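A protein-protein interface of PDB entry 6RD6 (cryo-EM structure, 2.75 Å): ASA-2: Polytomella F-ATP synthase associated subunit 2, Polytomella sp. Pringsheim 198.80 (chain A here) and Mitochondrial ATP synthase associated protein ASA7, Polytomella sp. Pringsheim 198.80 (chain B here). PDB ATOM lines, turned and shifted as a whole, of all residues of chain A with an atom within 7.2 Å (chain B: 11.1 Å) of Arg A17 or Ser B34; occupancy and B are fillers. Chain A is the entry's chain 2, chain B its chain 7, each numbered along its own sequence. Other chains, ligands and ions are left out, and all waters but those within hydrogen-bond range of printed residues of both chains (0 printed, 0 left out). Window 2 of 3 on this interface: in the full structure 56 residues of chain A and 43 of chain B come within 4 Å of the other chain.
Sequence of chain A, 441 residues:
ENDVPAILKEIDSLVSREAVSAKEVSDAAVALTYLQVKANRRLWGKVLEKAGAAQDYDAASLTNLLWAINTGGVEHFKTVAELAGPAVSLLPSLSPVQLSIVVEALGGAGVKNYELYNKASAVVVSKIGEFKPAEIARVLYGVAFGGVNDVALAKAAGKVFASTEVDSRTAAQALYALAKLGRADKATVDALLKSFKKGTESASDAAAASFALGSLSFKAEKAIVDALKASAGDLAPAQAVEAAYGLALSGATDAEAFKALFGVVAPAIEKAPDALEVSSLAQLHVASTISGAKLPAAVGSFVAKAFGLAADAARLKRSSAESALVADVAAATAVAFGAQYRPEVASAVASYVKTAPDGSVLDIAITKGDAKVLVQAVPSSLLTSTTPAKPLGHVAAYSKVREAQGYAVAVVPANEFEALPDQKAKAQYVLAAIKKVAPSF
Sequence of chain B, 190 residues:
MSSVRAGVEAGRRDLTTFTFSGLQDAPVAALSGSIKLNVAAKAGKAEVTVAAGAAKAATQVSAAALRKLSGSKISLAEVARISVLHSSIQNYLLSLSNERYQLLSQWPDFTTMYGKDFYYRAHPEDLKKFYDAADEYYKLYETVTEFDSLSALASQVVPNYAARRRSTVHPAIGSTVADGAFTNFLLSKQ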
ATOM      1  N   GLU A  10      19.623   1.965 -23.209  1.00  0.00           N
ATOM      2  CA  GLU A  10      19.950   2.595 -21.934  1.00  0.00           C
ATOM      3  C   GLU A  10      19.938   1.588 -20.790  1.00  0.00           C
ATOM      4  O   GLU A  10      20.753   1.685 -19.866  1.00  0.00           O
ATOM      5  CB  GLU A  10      18.989   3.746 -21.648  1.00  0.00           C
ATOM      6  CG  GLU A  10      19.331   5.012 -22.404  1.00  0.00           C
ATOM      7  CD  GLU A  10      20.437   5.804 -21.738  1.00  0.00           C
ATOM      8  OE1 GLU A  10      21.618   5.576 -22.075  1.00  0.00           O
ATOM      9  OE2 GLU A  10      20.130   6.647 -20.870  1.00  0.00           O
ATOM     10  N   ASP A  12      20.711  -1.605 -21.203  1.00  0.00           N
ATOM     11  CA  ASP A  12      21.922  -2.386 -21.430  1.00  0.00           C
ATOM     12  C   ASP A  12      23.168  -1.636 -20.985  1.00  0.00           C
ATOM     13  O   ASP A  12      24.130  -2.249 -20.515  1.00  0.00           O
ATOM     14  CB  ASP A  12      22.023  -2.767 -22.906  1.00  0.00           C
ATOM     15  CG  ASP A  12      23.195  -3.680 -23.194  1.00  0.00           C
ATOM     16  OD1 ASP A  12      23.035  -4.912 -23.070  1.00  0.00           O
ATOM     17  OD2 ASP A  12      24.275  -3.167 -23.549  1.00  0.00           O
ATOM     18  N   SER A  13      23.173  -0.309 -21.122  1.00  0.00           N
ATOM     19  CA  SER A  13      24.295   0.466 -20.601  1.00  0.00           C
ATOM     20  C   SER A  13      24.233   0.569 -19.082  1.00  0.00           C
ATOM     21  O   SER A  13      25.263   0.738 -18.422  1.00  0.00           O
ATOM     22  CB  SER A  13      24.319   1.854 -21.236  1.00  0.00           C
ATOM     23  OG  SER A  13      23.174   2.601 -20.869  1.00  0.00           O
ATOM     24  N   LEU A  14      23.030   0.482 -18.511  1.00  0.00           N
ATOM     25  CA  LEU A  14      22.889   0.514 -17.059  1.00  0.00           C
ATOM     26  C   LEU A  14      23.406  -0.766 -16.416  1.00  0.00           C
ATOM     27  O   LEU A  14      24.076  -0.720 -15.379  1.00  0.00           O
ATOM     28  CB  LEU A  14      21.424   0.743 -16.689  1.00  0.00           C
ATOM     29  CG  LEU A  14      20.989   0.462 -15.250  1.00  0.00           C
ATOM     30  CD1 LEU A  14      21.628   1.445 -14.301  1.00  0.00           C
ATOM     31  CD2 LEU A  14      19.479   0.506 -15.126  1.00  0.00           C
ATOM     32  N   VAL A  15      23.101  -1.925 -17.009  1.00  0.00           N
ATOM     33  CA  VAL A  15      23.503  -3.191 -16.403  1.00  0.00           C
ATOM     34  C   VAL A  15      24.870  -3.661 -16.871  1.00  0.00           C
ATOM     35  O   VAL A  15      25.274  -4.782 -16.537  1.00  0.00           O
ATOM     36  CB  VAL A  15      22.461  -4.299 -16.662  1.00  0.00           C
ATOM     37  CG1 VAL A  15      21.133  -3.925 -16.043  1.00  0.00           C
ATOM     38  CG2 VAL A  15      22.312  -4.559 -18.144  1.00  0.00           C
ATOM     39  N   SER A  16      25.598  -2.848 -17.628  1.00  0.00           N
ATOM     40  CA  SER A  16      26.958  -3.181 -18.025  1.00  0.00           C
ATOM     41  C   SER A  16      28.004  -2.459 -17.190  1.00  0.00           C
ATOM     42  O   SER A  16      29.192  -2.524 -17.518  1.00  0.00           O
ATOM     43  CB  SER A  16      27.174  -2.859 -19.502  1.00  0.00           C
ATOM     44  OG  SER A  16      26.322  -3.641 -20.316  1.00  0.00           O
ATOM     45  N   ARG A  17      27.594  -1.782 -16.125  1.00  0.00           N
ATOM     46  CA  ARG A  17      28.519  -0.991 -15.332  1.00  0.00           C
ATOM     47  C   ARG A  17      29.320  -1.866 -14.376  1.00  0.00           C
ATOM     48  O   ARG A  17      29.115  -3.077 -14.280  1.00  0.00           O
ATOM     49  CB  ARG A  17      27.759   0.077 -14.557  1.00  0.00           C
ATOM     50  CG  ARG A  17      26.913   0.957 -15.445  1.00  0.00           C
ATOM     51  CD  ARG A  17      26.886   2.377 -14.943  1.00  0.00           C
ATOM     52  NE  ARG A  17      26.002   2.528 -13.795  1.00  0.00           N
ATOM     53  CZ  ARG A  17      24.833   3.154 -13.837  1.00  0.00           C
ATOM     54  NH1 ARG A  17      24.407   3.687 -14.972  1.00  0.00           N
ATOM     55  NH2 ARG A  17      24.091   3.248 -12.744  1.00  0.00           N
ATOM     56  N   GLU A  18      30.250  -1.229 -13.663  1.00  0.00           N
ATOM     57  CA  GLU A  18      31.128  -1.970 -12.766  1.00  0.00           C
ATOM     58  C   GLU A  18      30.415  -2.323 -11.466  1.00  0.00           C
ATOM     59  O   GLU A  18      30.609  -3.415 -10.920  1.00  0.00           O
ATOM     60  CB  GLU A  18      32.389  -1.152 -12.487  1.00  0.00           C
ATOM     61  CG  GLU A  18      33.472  -1.887 -11.710  1.00  0.00           C
ATOM     62  CD  GLU A  18      34.151  -2.977 -12.525  1.00  0.00           C
ATOM     63  OE1 GLU A  18      34.195  -2.858 -13.767  1.00  0.00           O
ATOM     64  OE2 GLU A  18      34.643  -3.954 -11.923  1.00  0.00           O
ATOM     65  N   ALA A  19      29.588  -1.414 -10.956  1.00  0.00           N
ATOM     66  CA  ALA A  19      28.870  -1.611  -9.703  1.00  0.00           C
ATOM     67  C   ALA A  19      27.412  -1.227  -9.897  1.00  0.00           C
ATOM     68  O   ALA A  19      27.085  -0.038  -9.968  1.00  0.00           O
ATOM     69  CB  ALA A  19      29.494  -0.788  -8.573  1.00  0.00           C
ATOM     70  N   VAL A  20      26.543  -2.229  -9.978  1.00  0.00           N
ATOM     71  CA  VAL A  20      25.109  -2.030 -10.135  1.00  0.00           C
ATOM     72  C   VAL A  20      24.425  -2.541  -8.875  1.00  0.00           C
ATOM     73  O   VAL A  20      24.529  -3.729  -8.548  1.00  0.00           O
ATOM     74  CB  VAL A  20      24.566  -2.753 -11.383  1.00  0.00           C
ATOM     75  CG1 VAL A  20      23.217  -2.201 -11.762  1.00  0.00           C
ATOM     76  CG2 VAL A  20      25.529  -2.620 -12.545  1.00  0.00           C
ATOM     77  N   SER A  21      23.735  -1.650  -8.169  1.00  0.00           N
ATOM     78  CA  SER A  21      23.062  -2.036  -6.939  1.00  0.00           C
ATOM     79  C   SER A  21      21.811  -2.845  -7.252  1.00  0.00           C
ATOM     80  O   SER A  21      21.340  -2.887  -8.388  1.00  0.00           O
ATOM     81  CB  SER A  21      22.691  -0.808  -6.109  1.00  0.00           C
ATOM     82  OG  SER A  21      21.772   0.019  -6.801  1.00  0.00           O
ATOM     83  N   GLU A  24      18.796  -1.053  -8.885  1.00  0.00           N
ATOM     84  CA  GLU A  24      18.918  -0.809 -10.318  1.00  0.00           C
ATOM     85  C   GLU A  24      18.682  -2.078 -11.125  1.00  0.00           C
ATOM     86  O   GLU A  24      18.047  -2.031 -12.184  1.00  0.00           O
ATOM     87  CB  GLU A  24      20.293  -0.226 -10.632  1.00  0.00           C
ATOM     88  CG  GLU A  24      20.673   0.962  -9.777  1.00  0.00           C
ATOM     89  CD  GLU A  24      22.087   1.433 -10.032  1.00  0.00           C
ATOM     90  OE1 GLU A  24      22.638   1.115 -11.106  1.00  0.00           O
ATOM     91  OE2 GLU A  24      22.654   2.119  -9.157  1.00  0.00           O
ATOM     92  N   ASP A  27      14.930  -2.805 -10.989  1.00  0.00           N
ATOM     93  CA  ASP A  27      14.183  -1.913 -11.867  1.00  0.00           C
ATOM     94  C   ASP A  27      14.428  -2.234 -13.335  1.00  0.00           C
ATOM     95  O   ASP A  27      13.513  -2.118 -14.160  1.00  0.00           O
ATOM     96  CB  ASP A  27      14.549  -0.468 -11.565  1.00  0.00           C
ATOM     97  CG  ASP A  27      14.060  -0.031 -10.214  1.00  0.00           C
ATOM     98  OD1 ASP A  27      13.070  -0.614  -9.727  1.00  0.00           O
ATOM     99  OD2 ASP A  27      14.651   0.902  -9.637  1.00  0.00           O
ATOM    100  N   LYS A  50      23.955  -9.394 -13.133  1.00  0.00           N
ATOM    101  CA  LYS A  50      24.044  -8.342 -12.130  1.00  0.00           C
ATOM    102  C   LYS A  50      23.138  -8.628 -10.939  1.00  0.00           C
ATOM    103  O   LYS A  50      23.375  -8.122  -9.838  1.00  0.00           O
ATOM    104  CB  LYS A  50      23.708  -6.996 -12.762  1.00  0.00           C
ATOM    105  CG  LYS A  50      24.755  -6.502 -13.728  1.00  0.00           C
ATOM    106  CD  LYS A  50      26.095  -6.330 -13.040  1.00  0.00           C
ATOM    107  CE  LYS A  50      27.180  -5.991 -14.039  1.00  0.00           C
ATOM    108  NZ  LYS A  50      28.436  -5.572 -13.370  1.00  0.00           N
ATOM    109  N   ALA B  29       6.186   1.259  -9.294  1.00  0.00           N
ATOM    110  CA  ALA B  29       7.196   2.302  -9.242  1.00  0.00           C
ATOM    111  C   ALA B  29       8.586   1.692  -9.214  1.00  0.00           C
ATOM    112  O   ALA B  29       8.794   0.617  -8.646  1.00  0.00           O
ATOM    113  CB  ALA B  29       7.003   3.195  -8.014  1.00  0.00           C
ATOM    114  N   ALA B  30       9.532   2.389  -9.834  1.00  0.00           N
ATOM    115  CA  ALA B  30      10.928   1.995  -9.755  1.00  0.00           C
ATOM    116  C   ALA B  30      11.526   2.437  -8.426  1.00  0.00           C
ATOM    117  O   ALA B  30      11.022   3.343  -7.760  1.00  0.00           O
ATOM    118  CB  ALA B  30      11.717   2.597 -10.913  1.00  0.00           C
ATOM    119  N   LEU B  31      12.618   1.784  -8.042  1.00  0.00           N
ATOM    120  CA  LEU B  31      13.266   2.018  -6.762  1.00  0.00           C
ATOM    121  C   LEU B  31      14.593   2.749  -6.893  1.00  0.00           C
ATOM    122  O   LEU B  31      15.145   3.187  -5.880  1.00  0.00           O
ATOM    123  CB  LEU B  31      13.482   0.686  -6.046  1.00  0.00           C
ATOM    124  CG  LEU B  31      12.207  -0.108  -5.780  1.00  0.00           C
ATOM    125  CD1 LEU B  31      12.559  -1.515  -5.389  1.00  0.00           C
ATOM    126  CD2 LEU B  31      11.380   0.554  -4.695  1.00  0.00           C
ATOM    127  N   SER B  32      15.118   2.887  -8.106  1.00  0.00           N
ATOM    128  CA  SER B  32      16.382   3.564  -8.338  1.00  0.00           C
ATOM    129  C   SER B  32      16.153   4.781  -9.220  1.00  0.00           C
ATOM    130  O   SER B  32      15.190   4.840  -9.989  1.00  0.00           O
ATOM    131  CB  SER B  32      17.405   2.636  -8.996  1.00  0.00           C
ATOM    132  OG  SER B  32      17.010   2.300 -10.313  1.00  0.00           O
ATOM    133  N   GLY B  33      17.054   5.757  -9.101  1.00  0.00           N
ATOM    134  CA  GLY B  33      16.965   6.951  -9.920  1.00  0.00           C
ATOM    135  C   GLY B  33      17.543   6.804 -11.309  1.00  0.00           C
ATOM    136  O   GLY B  33      17.393   7.713 -12.129  1.00  0.00           O
ATOM    137  N   SER B  34      18.199   5.677 -11.591  1.00  0.00           N
ATOM    138  CA  SER B  34      18.831   5.491 -12.894  1.00  0.00           C
ATOM    139  C   SER B  34      17.799   5.196 -13.973  1.00  0.00           C
ATOM    140  O   SER B  34      18.073   5.357 -15.167  1.00  0.00           O
ATOM    141  CB  SER B  34      19.858   4.364 -12.817  1.00  0.00           C
ATOM    142  OG  SER B  34      20.899   4.682 -11.911  1.00  0.00           O
ATOM    143  N   ILE B  35      16.612   4.757 -13.572  1.00  0.00           N
ATOM    144  CA  ILE B  35      15.541   4.396 -14.489  1.00  0.00           C
ATOM    145  C   ILE B  35      14.216   4.620 -13.772  1.00  0.00           C
ATOM    146  O   ILE B  35      14.045   4.193 -12.626  1.00  0.00           O
ATOM    147  CB  ILE B  35      15.697   2.943 -14.985  1.00  0.00           C
ATOM    148  CG1 ILE B  35      14.456   2.454 -15.725  1.00  0.00           C
ATOM    149  CG2 ILE B  35      16.113   2.003 -13.859  1.00  0.00           C
ATOM    150  CD1 ILE B  35      14.698   1.166 -16.458  1.00  0.00           C
ATOM    151  N   LYS B  36      13.302   5.329 -14.426  1.00  0.00           N
ATOM    152  CA  LYS B  36      12.047   5.763 -13.829  1.00  0.00           C
ATOM    153  C   LYS B  36      10.890   5.013 -14.468  1.00  0.00           C
ATOM    154  O   LYS B  36      10.762   4.987 -15.696  1.00  0.00           O
ATOM    155  CB  LYS B  36      11.859   7.270 -13.999  1.00  0.00           C
ATOM    156  CG  LYS B  36      12.510   8.103 -12.913  1.00  0.00           C
ATOM    157  CD  LYS B  36      12.910   9.468 -13.437  1.00  0.00           C
ATOM    158  CE  LYS B  36      14.272   9.421 -14.105  1.00  0.00           C
ATOM    159  NZ  LYS B  36      15.331   8.944 -13.173  1.00  0.00           N
ATOM    160  N   LEU B  37      10.051   4.415 -13.629  1.00  0.00           N
ATOM    161  CA  LEU B  37       8.915   3.613 -14.064  1.00  0.00           C
ATOM    162  C   LEU B  37       7.643   4.220 -13.501  1.00  0.00           C
ATOM    163  O   LEU B  37       7.544   4.442 -12.291  1.00  0.00           O
ATOM    164  CB  LEU B  37       9.046   2.166 -13.588  1.00  0.00           C
ATOM    165  CG  LEU B  37       7.846   1.282 -13.923  1.00  0.00           C
ATOM    166  CD1 LEU B  37       7.769   0.952 -15.399  1.00  0.00           C
ATOM    167  CD2 LEU B  37       7.846   0.044 -13.073  1.00  0.00           C
ATOM    168  N   THR B  49       5.269   3.692 -18.616  1.00  0.00           N
ATOM    169  CA  THR B  49       6.218   4.687 -19.093  1.00  0.00           C
ATOM    170  C   THR B  49       7.553   4.433 -18.404  1.00  0.00           C
ATOM    171  O   THR B  49       7.642   4.489 -17.170  1.00  0.00           O
ATOM    172  CB  THR B  49       5.733   6.110 -18.815  1.00  0.00           C
ATOM    173  OG1 THR B  49       5.356   6.226 -17.441  1.00  0.00           O
ATOM    174  CG2 THR B  49       4.537   6.458 -19.683  1.00  0.00           C
ATOM    175  N   VAL B  50       8.573   4.141 -19.204  1.00  0.00           N
ATOM    176  CA  VAL B  50       9.921   3.848 -18.733  1.00  0.00           C
ATOM    177  C   VAL B  50      10.849   4.910 -19.300  1.00  0.00           C
ATOM    178  O   VAL B  50      10.883   5.129 -20.516  1.00  0.00           O
ATOM    179  CB  VAL B  50      10.375   2.443 -19.157  1.00  0.00           C
ATOM    180  CG1 VAL B  50      11.747   2.128 -18.586  1.00  0.00           C
ATOM    181  CG2 VAL B  50       9.370   1.414 -18.711  1.00  0.00           C
ATOM    182  N   ALA B  51      11.609   5.566 -18.427  1.00  0.00           N
ATOM    183  CA  ALA B  51      12.505   6.641 -18.837  1.00  0.00           C
ATOM    184  C   ALA B  51      13.888   6.403 -18.254  1.00  0.00           C
ATOM    185  O   ALA B  51      14.030   6.219 -17.043  1.00  0.00           O
ATOM    186  CB  ALA B  51      11.964   8.002 -18.396  1.00  0.00           C
ATOM    187  N   ALA B  52      14.905   6.410 -19.110  1.00  0.00           N
ATOM    188  CA  ALA B  52      16.295   6.335 -18.682  1.00  0.00           C
ATOM    189  C   ALA B  52      17.114   7.267 -19.561  1.00  0.00           C
ATOM    190  O   ALA B  52      17.216   7.047 -20.774  1.00  0.00           O
ATOM    191  CB  ALA B  52      16.835   4.906 -18.755  1.00  0.00           C
ATOM    192  N   GLY B  53      17.678   8.305 -18.949  1.00  0.00           N
ATOM    193  CA  GLY B  53      18.464   9.277 -19.689  1.00  0.00           C
ATOM    194  C   GLY B  53      17.613  10.054 -20.668  1.00  0.00           C
ATOM    195  O   GLY B  53      16.570  10.618 -20.315  1.00  0.00           O
ATOM    196  N   ALA B  54      18.051  10.074 -21.926  1.00  0.00           N
ATOM    197  CA  ALA B  54      17.263  10.715 -22.969  1.00  0.00           C
ATOM    198  C   ALA B  54      16.217   9.762 -23.534  1.00  0.00           C
ATOM    199  O   ALA B  54      15.341  10.179 -24.300  1.00  0.00           O
ATOM    200  CB  ALA B  54      18.179  11.231 -24.077  1.00  0.00           C
ATOM    201  N   ALA B  55      16.293   8.482 -23.174  1.00  0.00           N
ATOM    202  CA  ALA B  55      15.381   7.504 -23.748  1.00  0.00           C
ATOM    203  C   ALA B  55      14.084   7.437 -22.955  1.00  0.00           C
ATOM    204  O   ALA B  55      14.089   7.400 -21.722  1.00  0.00           O
ATOM    205  CB  ALA B  55      16.040   6.129 -23.795  1.00  0.00           C
ATOM    206  N   LYS B  56      12.967   7.430 -23.676  1.00  0.00           N
ATOM    207  CA  LYS B  56      11.648   7.290 -23.079  1.00  0.00           C
ATOM    208  C   LYS B  56      10.836   6.303 -23.901  1.00  0.00           C
ATOM    209  O   LYS B  56      11.003   6.199 -25.118  1.00  0.00           O
ATOM    210  CB  LYS B  56      10.906   8.631 -22.994  1.00  0.00           C
ATOM    211  CG  LYS B  56      11.488   9.607 -21.990  1.00  0.00           C
ATOM    212  CD  LYS B  56      10.911  11.000 -22.167  1.00  0.00           C
ATOM    213  CE  LYS B  56      11.539  11.978 -21.190  1.00  0.00           C
ATOM    214  NZ  LYS B  56      11.427  11.500 -19.787  1.00  0.00           N
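The backbone NH (N) of Leu B31 lies within hydrogen-bond range of the side-chain carboxylate (OD2) of Asp A27 (2.7 Å). The side-chain carboxylate of Asp A27 sits at hydrogen-bond distance from the backbone NH of Ser B32, 2.5 Å away. O of Ala B52 sits close to OE2 of Glu A10 (2.9 Å).
The guanidinium group (NH2) of Arg A17 is in salt-bridge range of the side-chain carboxylate (OE1) of Glu A24, at 3.1 Å. The side-chain hydroxyl of Ser A13 is in hydrogen-bond range of the backbone carbonyl oxygen of Glu A10 (2.8 Å). The side-chain hydroxyl (OG) of Ser A21 sits at hydrogen-bond distance from the side-chain carboxylate (OE2) of Glu A24 (3.3 Å). The backbone carbonyl oxygen (O) of Arg A17 sits at hydrogen-bond distance from the side-chain amino group (NZ) of Lys A50 (2.7 Å).
Among the printed residues, merely in contact across the chains: Glu A10 with Gly B53 (3.3 Å), Asp A27 with Ala B30 (3.4 Å), Arg A17 with Ser B34 (3.6 Å), Glu A24 with Ser B32 (3.6 Å), Asp A27 with Ile B35 (3.7 Å), Leu A14 with Ser B34 (3.7 Å), Glu A10 with Ala B55 (3.7 Å), Leu A14 with Ile B35 (3.9 Å) and Glu A24 with Ser B34 (3.9 Å).
Of the printed residues of chain B, Glu A10 touches Ala B52, Gly B53 and Ala B55. No residue of chain B comes within 4 Å of Ser A13. Leu A14 touches just these residues of chain B: Ser B34 and Ile B35. No residue of chain B comes within 4 Å of Val A15. No residue of chain B comes within 4 Å of Ser A16. Arg A17 touches one residue of chain B. Of chain B, only Ser B32 (3.6 Å) and Ser B34 (3.9 Å) come within 4 Å of Glu A24. Printed residues of chain A within 4 Å of Ala B30: Asp A27. Of the printed residues of chain A, Ser B32 touches Glu A24 (3.6 Å) and Asp A27 (2.5 Å). No residue of chain A comes within 4 Å of Gly B33. Ser B34 touches just these residues of chain A: Leu A14, Arg A17 and Glu A24. Printed residues of chain A within 4 Å of Ile B35: Leu A14 and Asp A27.
Of the 14 printed residues of chain A, 5 touch a printed residue of chain B. Of the 17 printed residues of chain B, 8 touch a printed residue of chain A. Among the printed residues, no Asp or Glu carboxylate lies within 4 Å of a Lys or Arg side-chain nitrogen of the other chain.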
